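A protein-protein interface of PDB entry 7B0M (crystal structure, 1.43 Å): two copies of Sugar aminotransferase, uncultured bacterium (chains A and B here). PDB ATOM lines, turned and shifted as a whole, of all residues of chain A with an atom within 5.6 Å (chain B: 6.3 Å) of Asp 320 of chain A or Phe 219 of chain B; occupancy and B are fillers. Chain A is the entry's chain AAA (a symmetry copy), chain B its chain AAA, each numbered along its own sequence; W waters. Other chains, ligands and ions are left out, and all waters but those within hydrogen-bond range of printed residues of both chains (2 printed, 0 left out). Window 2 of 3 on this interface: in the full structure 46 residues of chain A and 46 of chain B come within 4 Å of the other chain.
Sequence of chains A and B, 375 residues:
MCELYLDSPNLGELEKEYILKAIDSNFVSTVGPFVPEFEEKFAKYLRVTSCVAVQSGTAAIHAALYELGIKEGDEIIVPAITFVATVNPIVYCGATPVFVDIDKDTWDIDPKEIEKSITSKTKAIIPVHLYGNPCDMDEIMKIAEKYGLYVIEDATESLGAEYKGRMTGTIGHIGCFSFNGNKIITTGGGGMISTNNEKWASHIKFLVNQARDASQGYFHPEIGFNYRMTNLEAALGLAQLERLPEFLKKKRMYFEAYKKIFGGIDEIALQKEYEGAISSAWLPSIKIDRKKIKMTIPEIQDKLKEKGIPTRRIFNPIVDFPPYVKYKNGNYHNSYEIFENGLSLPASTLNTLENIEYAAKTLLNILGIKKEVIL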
ATOM      1  N   ASN A 316       8.616 -23.258 -12.003  1.00  0.00           N
ATOM      2  CA  ASN A 316       7.251 -23.008 -11.509  1.00  0.00           C
ATOM      3  C   ASN A 316       7.017 -21.547 -11.224  1.00  0.00           C
ATOM      4  O   ASN A 316       7.843 -20.783 -10.660  1.00  0.00           O
ATOM      5  CB  ASN A 316       7.005 -23.774 -10.191  1.00  0.00           C
ATOM      6  CG  ASN A 316       6.474 -25.162 -10.377  1.00  0.00           C
ATOM      7  OD1 ASN A 316       7.152 -26.056 -10.830  1.00  0.00           O
ATOM      8  ND2 ASN A 316       5.225 -25.324  -9.956  1.00  0.00           N
ATOM      9  N   PRO A 317       5.786 -21.019 -11.390  1.00  0.00           N
ATOM     10  CA  PRO A 317       5.438 -19.689 -10.966  1.00  0.00           C
ATOM     11  C   PRO A 317       5.613 -19.538  -9.451  1.00  0.00           C
ATOM     12  O   PRO A 317       5.065 -20.347  -8.653  1.00  0.00           O
ATOM     13  CB  PRO A 317       3.921 -19.603 -11.298  1.00  0.00           C
ATOM     14  CG  PRO A 317       3.795 -20.527 -12.441  1.00  0.00           C
ATOM     15  CD  PRO A 317       4.674 -21.696 -12.103  1.00  0.00           C
ATOM     16  N   ILE A 318       6.447 -18.585  -9.060  1.00  0.00           N
ATOM     17  CA  ILE A 318       6.858 -18.450  -7.645  1.00  0.00           C
ATOM     18  C   ILE A 318       5.655 -18.038  -6.788  1.00  0.00           C
ATOM     19  O   ILE A 318       5.656 -18.358  -5.560  1.00  0.00           O
ATOM     20  CB  ILE A 318       8.072 -17.509  -7.515  1.00  0.00           C
ATOM     21  CG1 ILE A 318       9.203 -18.134  -8.321  1.00  0.00           C
ATOM     22  CG2 ILE A 318       8.399 -17.238  -6.060  1.00  0.00           C
ATOM     23  CD1 ILE A 318      10.462 -17.261  -8.438  1.00  0.00           C
ATOM     24  N   VAL A 319       4.686 -17.318  -7.371  1.00  0.00           N
ATOM     25  CA  VAL A 319       3.504 -16.814  -6.620  1.00  0.00           C
ATOM     26  C   VAL A 319       2.672 -18.010  -6.121  1.00  0.00           C
ATOM     27  O   VAL A 319       1.797 -17.704  -5.321  1.00  0.00           O
ATOM     28  CB  VAL A 319       2.654 -15.917  -7.536  1.00  0.00           C
ATOM     29  CG1 VAL A 319       3.381 -14.594  -7.786  1.00  0.00           C
ATOM     30  CG2 VAL A 319       2.293 -16.633  -8.807  1.00  0.00           C
ATOM     31  N   ASP A 320       2.939 -19.243  -6.537  1.00  0.00           N
ATOM     32  CA  ASP A 320       2.130 -20.376  -5.962  1.00  0.00           C
ATOM     33  C   ASP A 320       2.971 -21.154  -4.954  1.00  0.00           C
ATOM     34  O   ASP A 320       2.547 -22.211  -4.480  1.00  0.00           O
ATOM     35  CB  ASP A 320       1.528 -21.254  -7.020  1.00  0.00           C
ATOM     36  CG  ASP A 320       0.507 -20.507  -7.895  1.00  0.00           C
ATOM     37  OD1 ASP A 320      -0.329 -19.688  -7.348  1.00  0.00           O
ATOM     38  OD2 ASP A 320       0.610 -20.738  -9.081  1.00  0.00           O
ATOM     39  N   PHE A 321       4.119 -20.610  -4.550  1.00  0.00           N
ATOM     40  CA  PHE A 321       4.861 -21.214  -3.416  1.00  0.00           C
ATOM     41  C   PHE A 321       4.280 -20.647  -2.143  1.00  0.00           C
ATOM     42  O   PHE A 321       4.021 -19.455  -2.020  1.00  0.00           O
ATOM     43  CB  PHE A 321       6.355 -20.853  -3.466  1.00  0.00           C
ATOM     44  CG  PHE A 321       7.065 -21.328  -4.692  1.00  0.00           C
ATOM     45  CD1 PHE A 321       6.534 -22.241  -5.580  1.00  0.00           C
ATOM     46  CD2 PHE A 321       8.387 -20.897  -4.898  1.00  0.00           C
ATOM     47  CE1 PHE A 321       7.236 -22.656  -6.708  1.00  0.00           C
ATOM     48  CE2 PHE A 321       9.096 -21.360  -5.997  1.00  0.00           C
ATOM     49  CZ  PHE A 321       8.551 -22.217  -6.899  1.00  0.00           C
ATOM     50  N   PRO A 322       4.068 -21.503  -1.094  1.00  0.00           N
ATOM     51  CA  PRO A 322       3.421 -20.999   0.120  1.00  0.00           C
ATOM     52  C   PRO A 322       3.945 -19.721   0.720  1.00  0.00           C
ATOM     53  O   PRO A 322       3.189 -18.893   1.127  1.00  0.00           O
ATOM     54  CB  PRO A 322       3.546 -22.220   1.042  1.00  0.00           C
ATOM     55  CG  PRO A 322       3.524 -23.357   0.147  1.00  0.00           C
ATOM     56  CD  PRO A 322       4.248 -22.933  -1.132  1.00  0.00           C
ATOM     57  N   VAL A 325       2.684 -16.643  -1.764  1.00  0.00           N
ATOM     58  CA  VAL A 325       1.311 -16.464  -2.315  1.00  0.00           C
ATOM     59  C   VAL A 325       0.678 -15.194  -1.747  1.00  0.00           C
ATOM     60  O   VAL A 325      -0.171 -14.623  -2.451  1.00  0.00           O
ATOM     61  CB  VAL A 325       0.445 -17.725  -2.153  1.00  0.00           C
ATOM     62  CG1 VAL A 325       0.138 -17.960  -0.688  1.00  0.00           C
ATOM     63  CG2 VAL A 325      -0.821 -17.615  -2.976  1.00  0.00           C
ATOM     64  N   LYS A 328       0.795 -12.608  -4.476  1.00  0.00           N
ATOM     65  CA  LYS A 328       0.192 -12.913  -5.776  1.00  0.00           C
ATOM     66  C   LYS A 328      -0.825 -11.830  -6.072  1.00  0.00           C
ATOM     67  O   LYS A 328      -1.898 -11.873  -5.502  1.00  0.00           O
ATOM     68  CB  LYS A 328      -0.457 -14.285  -5.760  1.00  0.00           C
ATOM     69  CG  LYS A 328      -0.972 -14.749  -7.091  1.00  0.00           C
ATOM     70  CD  LYS A 328      -1.432 -16.161  -7.113  1.00  0.00           C
ATOM     71  CE  LYS A 328      -1.929 -16.558  -8.483  1.00  0.00           C
ATOM     72  NZ  LYS A 328      -2.473 -17.933  -8.456  1.00  0.00           N
ATOM     73  N   TYR A 336       1.793 -18.309 -16.541  1.00  0.00           N
ATOM     74  CA  TYR A 336       1.126 -19.625 -16.538  1.00  0.00           C
ATOM     75  C   TYR A 336       1.134 -20.323 -17.884  1.00  0.00           C
ATOM     76  O   TYR A 336       1.342 -21.509 -17.972  1.00  0.00           O
ATOM     77  CB  TYR A 336      -0.322 -19.472 -16.015  1.00  0.00           C
ATOM     78  CG  TYR A 336      -0.418 -19.344 -14.527  1.00  0.00           C
ATOM     79  CD1 TYR A 336       0.033 -20.348 -13.660  1.00  0.00           C
ATOM     80  CD2 TYR A 336      -0.933 -18.215 -13.980  1.00  0.00           C
ATOM     81  CE1 TYR A 336      -0.025 -20.203 -12.284  1.00  0.00           C
ATOM     82  CE2 TYR A 336      -0.982 -18.043 -12.609  1.00  0.00           C
ATOM     83  CZ  TYR A 336      -0.510 -19.028 -11.748  1.00  0.00           C
ATOM     84  OH  TYR A 336      -0.622 -18.736 -10.412  1.00  0.00           O
ATOM     85  N   ALA B 211      15.501 -25.697  -0.394  1.00  0.00           N
ATOM     86  CA  ALA B 211      14.133 -26.145  -0.031  1.00  0.00           C
ATOM     87  C   ALA B 211      13.365 -26.633  -1.269  1.00  0.00           C
ATOM     88  O   ALA B 211      12.175 -26.255  -1.393  1.00  0.00           O
ATOM     89  CB  ALA B 211      13.447 -25.092   0.722  1.00  0.00           C
ATOM     90  N   ARG B 212      13.990 -27.311  -2.186  1.00  0.00           N
ATOM     91  CA  ARG B 212      13.364 -27.816  -3.438  1.00  0.00           C
ATOM     92  C   ARG B 212      12.662 -29.144  -3.103  1.00  0.00           C
ATOM     93  O   ARG B 212      13.326 -30.039  -2.554  1.00  0.00           O
ATOM     94  CB  ARG B 212      14.366 -27.934  -4.573  1.00  0.00           C
ATOM     95  CG  ARG B 212      13.642 -28.107  -5.912  1.00  0.00           C
ATOM     96  CD  ARG B 212      14.544 -28.334  -7.102  1.00  0.00           C
ATOM     97  NE  ARG B 212      15.214 -29.619  -7.010  1.00  0.00           N
ATOM     98  CZ  ARG B 212      14.721 -30.824  -7.350  1.00  0.00           C
ATOM     99  NH1 ARG B 212      13.488 -30.974  -7.806  1.00  0.00           N
ATOM    100  NH2 ARG B 212      15.481 -31.900  -7.229  1.00  0.00           N
ATOM    101  N   ASP B 213      11.389 -29.288  -3.469  1.00  0.00           N
ATOM    102  CA  ASP B 213      10.692 -30.582  -3.363  1.00  0.00           C
ATOM    103  C   ASP B 213      11.289 -31.499  -4.412  1.00  0.00           C
ATOM    104  O   ASP B 213      10.984 -31.283  -5.632  1.00  0.00           O
ATOM    105  CB  ASP B 213       9.197 -30.409  -3.642  1.00  0.00           C
ATOM    106  CG  ASP B 213       8.426 -31.665  -3.310  1.00  0.00           C
ATOM    107  OD1 ASP B 213       9.030 -32.739  -3.444  1.00  0.00           O
ATOM    108  OD2 ASP B 213       7.257 -31.567  -2.899  1.00  0.00           O
ATOM    109  N   ALA B 214      11.955 -32.539  -3.983  1.00  0.00           N
ATOM    110  CA  ALA B 214      12.660 -33.524  -4.857  1.00  0.00           C
ATOM    111  C   ALA B 214      11.682 -34.315  -5.739  1.00  0.00           C
ATOM    112  O   ALA B 214      12.106 -34.855  -6.786  1.00  0.00           O
ATOM    113  CB  ALA B 214      13.502 -34.462  -4.011  1.00  0.00           C
ATOM    114  N   GLN B 216       9.100 -33.035  -7.211  1.00  0.00           N
ATOM    115  CA  GLN B 216       8.561 -32.156  -8.260  1.00  0.00           C
ATOM    116  C   GLN B 216       9.782 -31.742  -9.096  1.00  0.00           C
ATOM    117  O   GLN B 216      10.904 -32.352  -8.895  1.00  0.00           O
ATOM    118  CB  GLN B 216       7.808 -30.957  -7.677  1.00  0.00           C
ATOM    119  CG  GLN B 216       6.834 -31.300  -6.543  1.00  0.00           C
ATOM    120  CD  GLN B 216       5.644 -32.106  -7.010  1.00  0.00           C
ATOM    121  OE1 GLN B 216       4.905 -31.663  -7.886  1.00  0.00           O
ATOM    122  NE2 GLN B 216       5.444 -33.282  -6.421  1.00  0.00           N
ATOM    123  N   GLY B 217       9.597 -30.766  -9.982  1.00  0.00           N
ATOM    124  CA  GLY B 217      10.717 -30.049 -10.639  1.00  0.00           C
ATOM    125  C   GLY B 217      11.110 -28.850  -9.785  1.00  0.00           C
ATOM    126  O   GLY B 217      11.436 -29.022  -8.567  1.00  0.00           O
ATOM    127  N   TYR B 218      10.901 -27.645 -10.293  1.00  0.00           N
ATOM    128  CA  TYR B 218      11.265 -26.421  -9.540  1.00  0.00           C
ATOM    129  C   TYR B 218      10.108 -25.912  -8.714  1.00  0.00           C
ATOM    130  O   TYR B 218       9.684 -24.776  -8.824  1.00  0.00           O
ATOM    131  CB  TYR B 218      11.758 -25.358 -10.516  1.00  0.00           C
ATOM    132  CG  TYR B 218      13.066 -25.685 -11.162  1.00  0.00           C
ATOM    133  CD1 TYR B 218      14.248 -25.740 -10.445  1.00  0.00           C
ATOM    134  CD2 TYR B 218      13.090 -25.867 -12.524  1.00  0.00           C
ATOM    135  CE1 TYR B 218      15.454 -26.013 -11.082  1.00  0.00           C
ATOM    136  CE2 TYR B 218      14.276 -26.096 -13.182  1.00  0.00           C
ATOM    137  CZ  TYR B 218      15.445 -26.216 -12.464  1.00  0.00           C
ATOM    138  OH  TYR B 218      16.553 -26.407 -13.244  1.00  0.00           O
ATOM    139  N   PHE B 219       9.740 -26.721  -7.716  1.00  0.00           N
ATOM    140  CA  PHE B 219       8.720 -26.345  -6.707  1.00  0.00           C
ATOM    141  C   PHE B 219       9.361 -26.293  -5.311  1.00  0.00           C
ATOM    142  O   PHE B 219      10.025 -27.267  -4.938  1.00  0.00           O
ATOM    143  CB  PHE B 219       7.500 -27.311  -6.705  1.00  0.00           C
ATOM    144  CG  PHE B 219       6.464 -26.832  -5.730  1.00  0.00           C
ATOM    145  CD1 PHE B 219       5.571 -25.816  -6.031  1.00  0.00           C
ATOM    146  CD2 PHE B 219       6.475 -27.326  -4.426  1.00  0.00           C
ATOM    147  CE1 PHE B 219       4.708 -25.288  -5.051  1.00  0.00           C
ATOM    148  CE2 PHE B 219       5.614 -26.779  -3.473  1.00  0.00           C
ATOM    149  CZ  PHE B 219       4.743 -25.787  -3.794  1.00  0.00           C
ATOM    150  N   HIS B 220       9.197 -25.156  -4.611  1.00  0.00           N
ATOM    151  CA  HIS B 220       9.840 -24.915  -3.306  1.00  0.00           C
ATOM    152  C   HIS B 220       8.777 -24.565  -2.282  1.00  0.00           C
ATOM    153  O   HIS B 220       8.224 -23.484  -2.288  1.00  0.00           O
ATOM    154  CB  HIS B 220      10.902 -23.816  -3.460  1.00  0.00           C
ATOM    155  CG  HIS B 220      11.851 -24.087  -4.551  1.00  0.00           C
ATOM    156  ND1 HIS B 220      13.158 -24.492  -4.347  1.00  0.00           N
ATOM    157  CD2 HIS B 220      11.725 -23.940  -5.907  1.00  0.00           C
ATOM    158  CE1 HIS B 220      13.783 -24.585  -5.523  1.00  0.00           C
ATOM    159  NE2 HIS B 220      12.887 -24.306  -6.506  1.00  0.00           N
ATOM    160  N   PRO B 221       8.541 -25.484  -1.290  1.00  0.00           N
ATOM    161  CA  PRO B 221       7.448 -25.260  -0.363  1.00  0.00           C
ATOM    162  C   PRO B 221       7.769 -24.276   0.721  1.00  0.00           C
ATOM    163  O   PRO B 221       6.880 -23.772   1.355  1.00  0.00           O
ATOM    164  CB  PRO B 221       7.224 -26.637   0.249  1.00  0.00           C
ATOM    165  CG  PRO B 221       8.494 -27.379   0.012  1.00  0.00           C
ATOM    166  CD  PRO B 221       8.989 -26.878  -1.323  1.00  0.00           C
ATOM    167  N   GLU B 222       9.094 -23.941   0.870  1.00  0.00           N
ATOM    168  CA  GLU B 222       9.445 -22.870   1.832  1.00  0.00           C
ATOM    169  C   GLU B 222      10.721 -22.154   1.343  1.00  0.00           C
ATOM    170  O   GLU B 222      11.282 -22.584   0.296  1.00  0.00           O
ATOM    171  CB  GLU B 222       9.635 -23.385   3.272  1.00  0.00           C
ATOM    172  CG  GLU B 222      10.712 -24.454   3.436  1.00  0.00           C
ATOM    173  CD  GLU B 222      10.726 -25.097   4.824  1.00  0.00           C
ATOM    174  OE1 GLU B 222      10.426 -26.338   4.917  1.00  0.00           O
ATOM    175  OE2 GLU B 222      11.015 -24.352   5.809  1.00  0.00           O
HETATM  176  O   HOH W   1       9.100 -26.754 -12.605  1.00  0.00           O
HETATM  177  O   HOH W   2       6.882 -28.779 -10.291  1.00  0.00           O
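Water W1 lies within hydrogen-bond range of OD1 of Asn 316 of chain A (2.7 Å) and N of Tyr 218 of chain B (3.1 Å).
Water W2 bridges the side-chain amide oxygen of Asn 316 of chain A (2.8 Å) and the backbone NH of Gly 217 of chain B (3.4 Å).
Asp 320 of chain A touches just one residue of chain B: Phe 219 (3.8 Å).
Phe 219 of chain B touches just these residues of chain A: Asn 316 (3.97 Å), Asp 320 (3.8 Å), Phe 321 (3.6 Å) and Pro 322 (3.9 Å).
Of the printed residues of chain B, Pro 322 of chain A touches Phe 219 and Pro 221.
Of the printed residues of chain A, His 220 of chain B touches Phe 321 (3.4 Å).
Of the printed residues of chain A, Tyr 218 of chain B touches Asn 316 and Phe 321.
Of the printed residues of chain A, Pro 221 of chain B touches Pro 322.
Printed residues of chain B within 4 Å of Asn 316 of chain A: Tyr 218 (3.2 Å) and Phe 219 (3.97 Å).
Pro 317 of chain A touches none of the printed residues of chain B.
The nearest residue of chain B that does not touch Asp 320 of chain A is His 220 of chain B (6.2 Å).
The nearest printed residue of chain A that does not touch Phe 219 of chain B is Pro 317 of chain A (6.1 Å).
CD1 of Phe 219 of chain B touches ND2 of Asn 316 of chain A, at 3.97 Å.
O of Asp 320 of chain A touches CE1 of Phe 219 of chain B, at 3.8 Å.
Phe 321 of chain A touches Tyr 218 of chain B (CZ to O, 3.4 Å).
Phe 321 of chain A touches Phe 219 of chain B.
CG of Phe 321 of chain A touches O of His 220 of chain B, at 3.4 Å.
Phe 219 of chain B touches Pro 322 of chain A.
Pro 322 of chain A touches Pro 221 of chain B (CG to O, 3.6 Å).
The backbone carbonyl oxygen (O) of Tyr 218 of chain B sits close to the side-chain amide oxygen (OD1) of Asn 316 of chain A, at 3.5 Å.
No position is printed for both chains.
Of the 8 pairs that touch across the chains among the printed residues, none has its exchanged pair printed and touching as well.
The backbone NH of Asp 213 of chain B is in hydrogen-bond range of the backbone carbonyl oxygen of Phe 219 of chain B (2.8 Å).
The side-chain carboxylate (OD1) of Asp 320 of chain A is in salt-bridge range of the side-chain amino group (NZ) of Lys 328 of chain A, 3.0 Å away.
OD2 of Asp 320 of chain A lies within hydrogen-bond range of OH of Tyr 336 of chain A, 2.7 Å away.
Of the 10 printed residues of chain A, 4 touch a printed residue of chain B.
Among the printed residues, no Asp or Glu carboxylate lies within 4 Å of a Lys or Arg side-chain nitrogen of the other chain.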
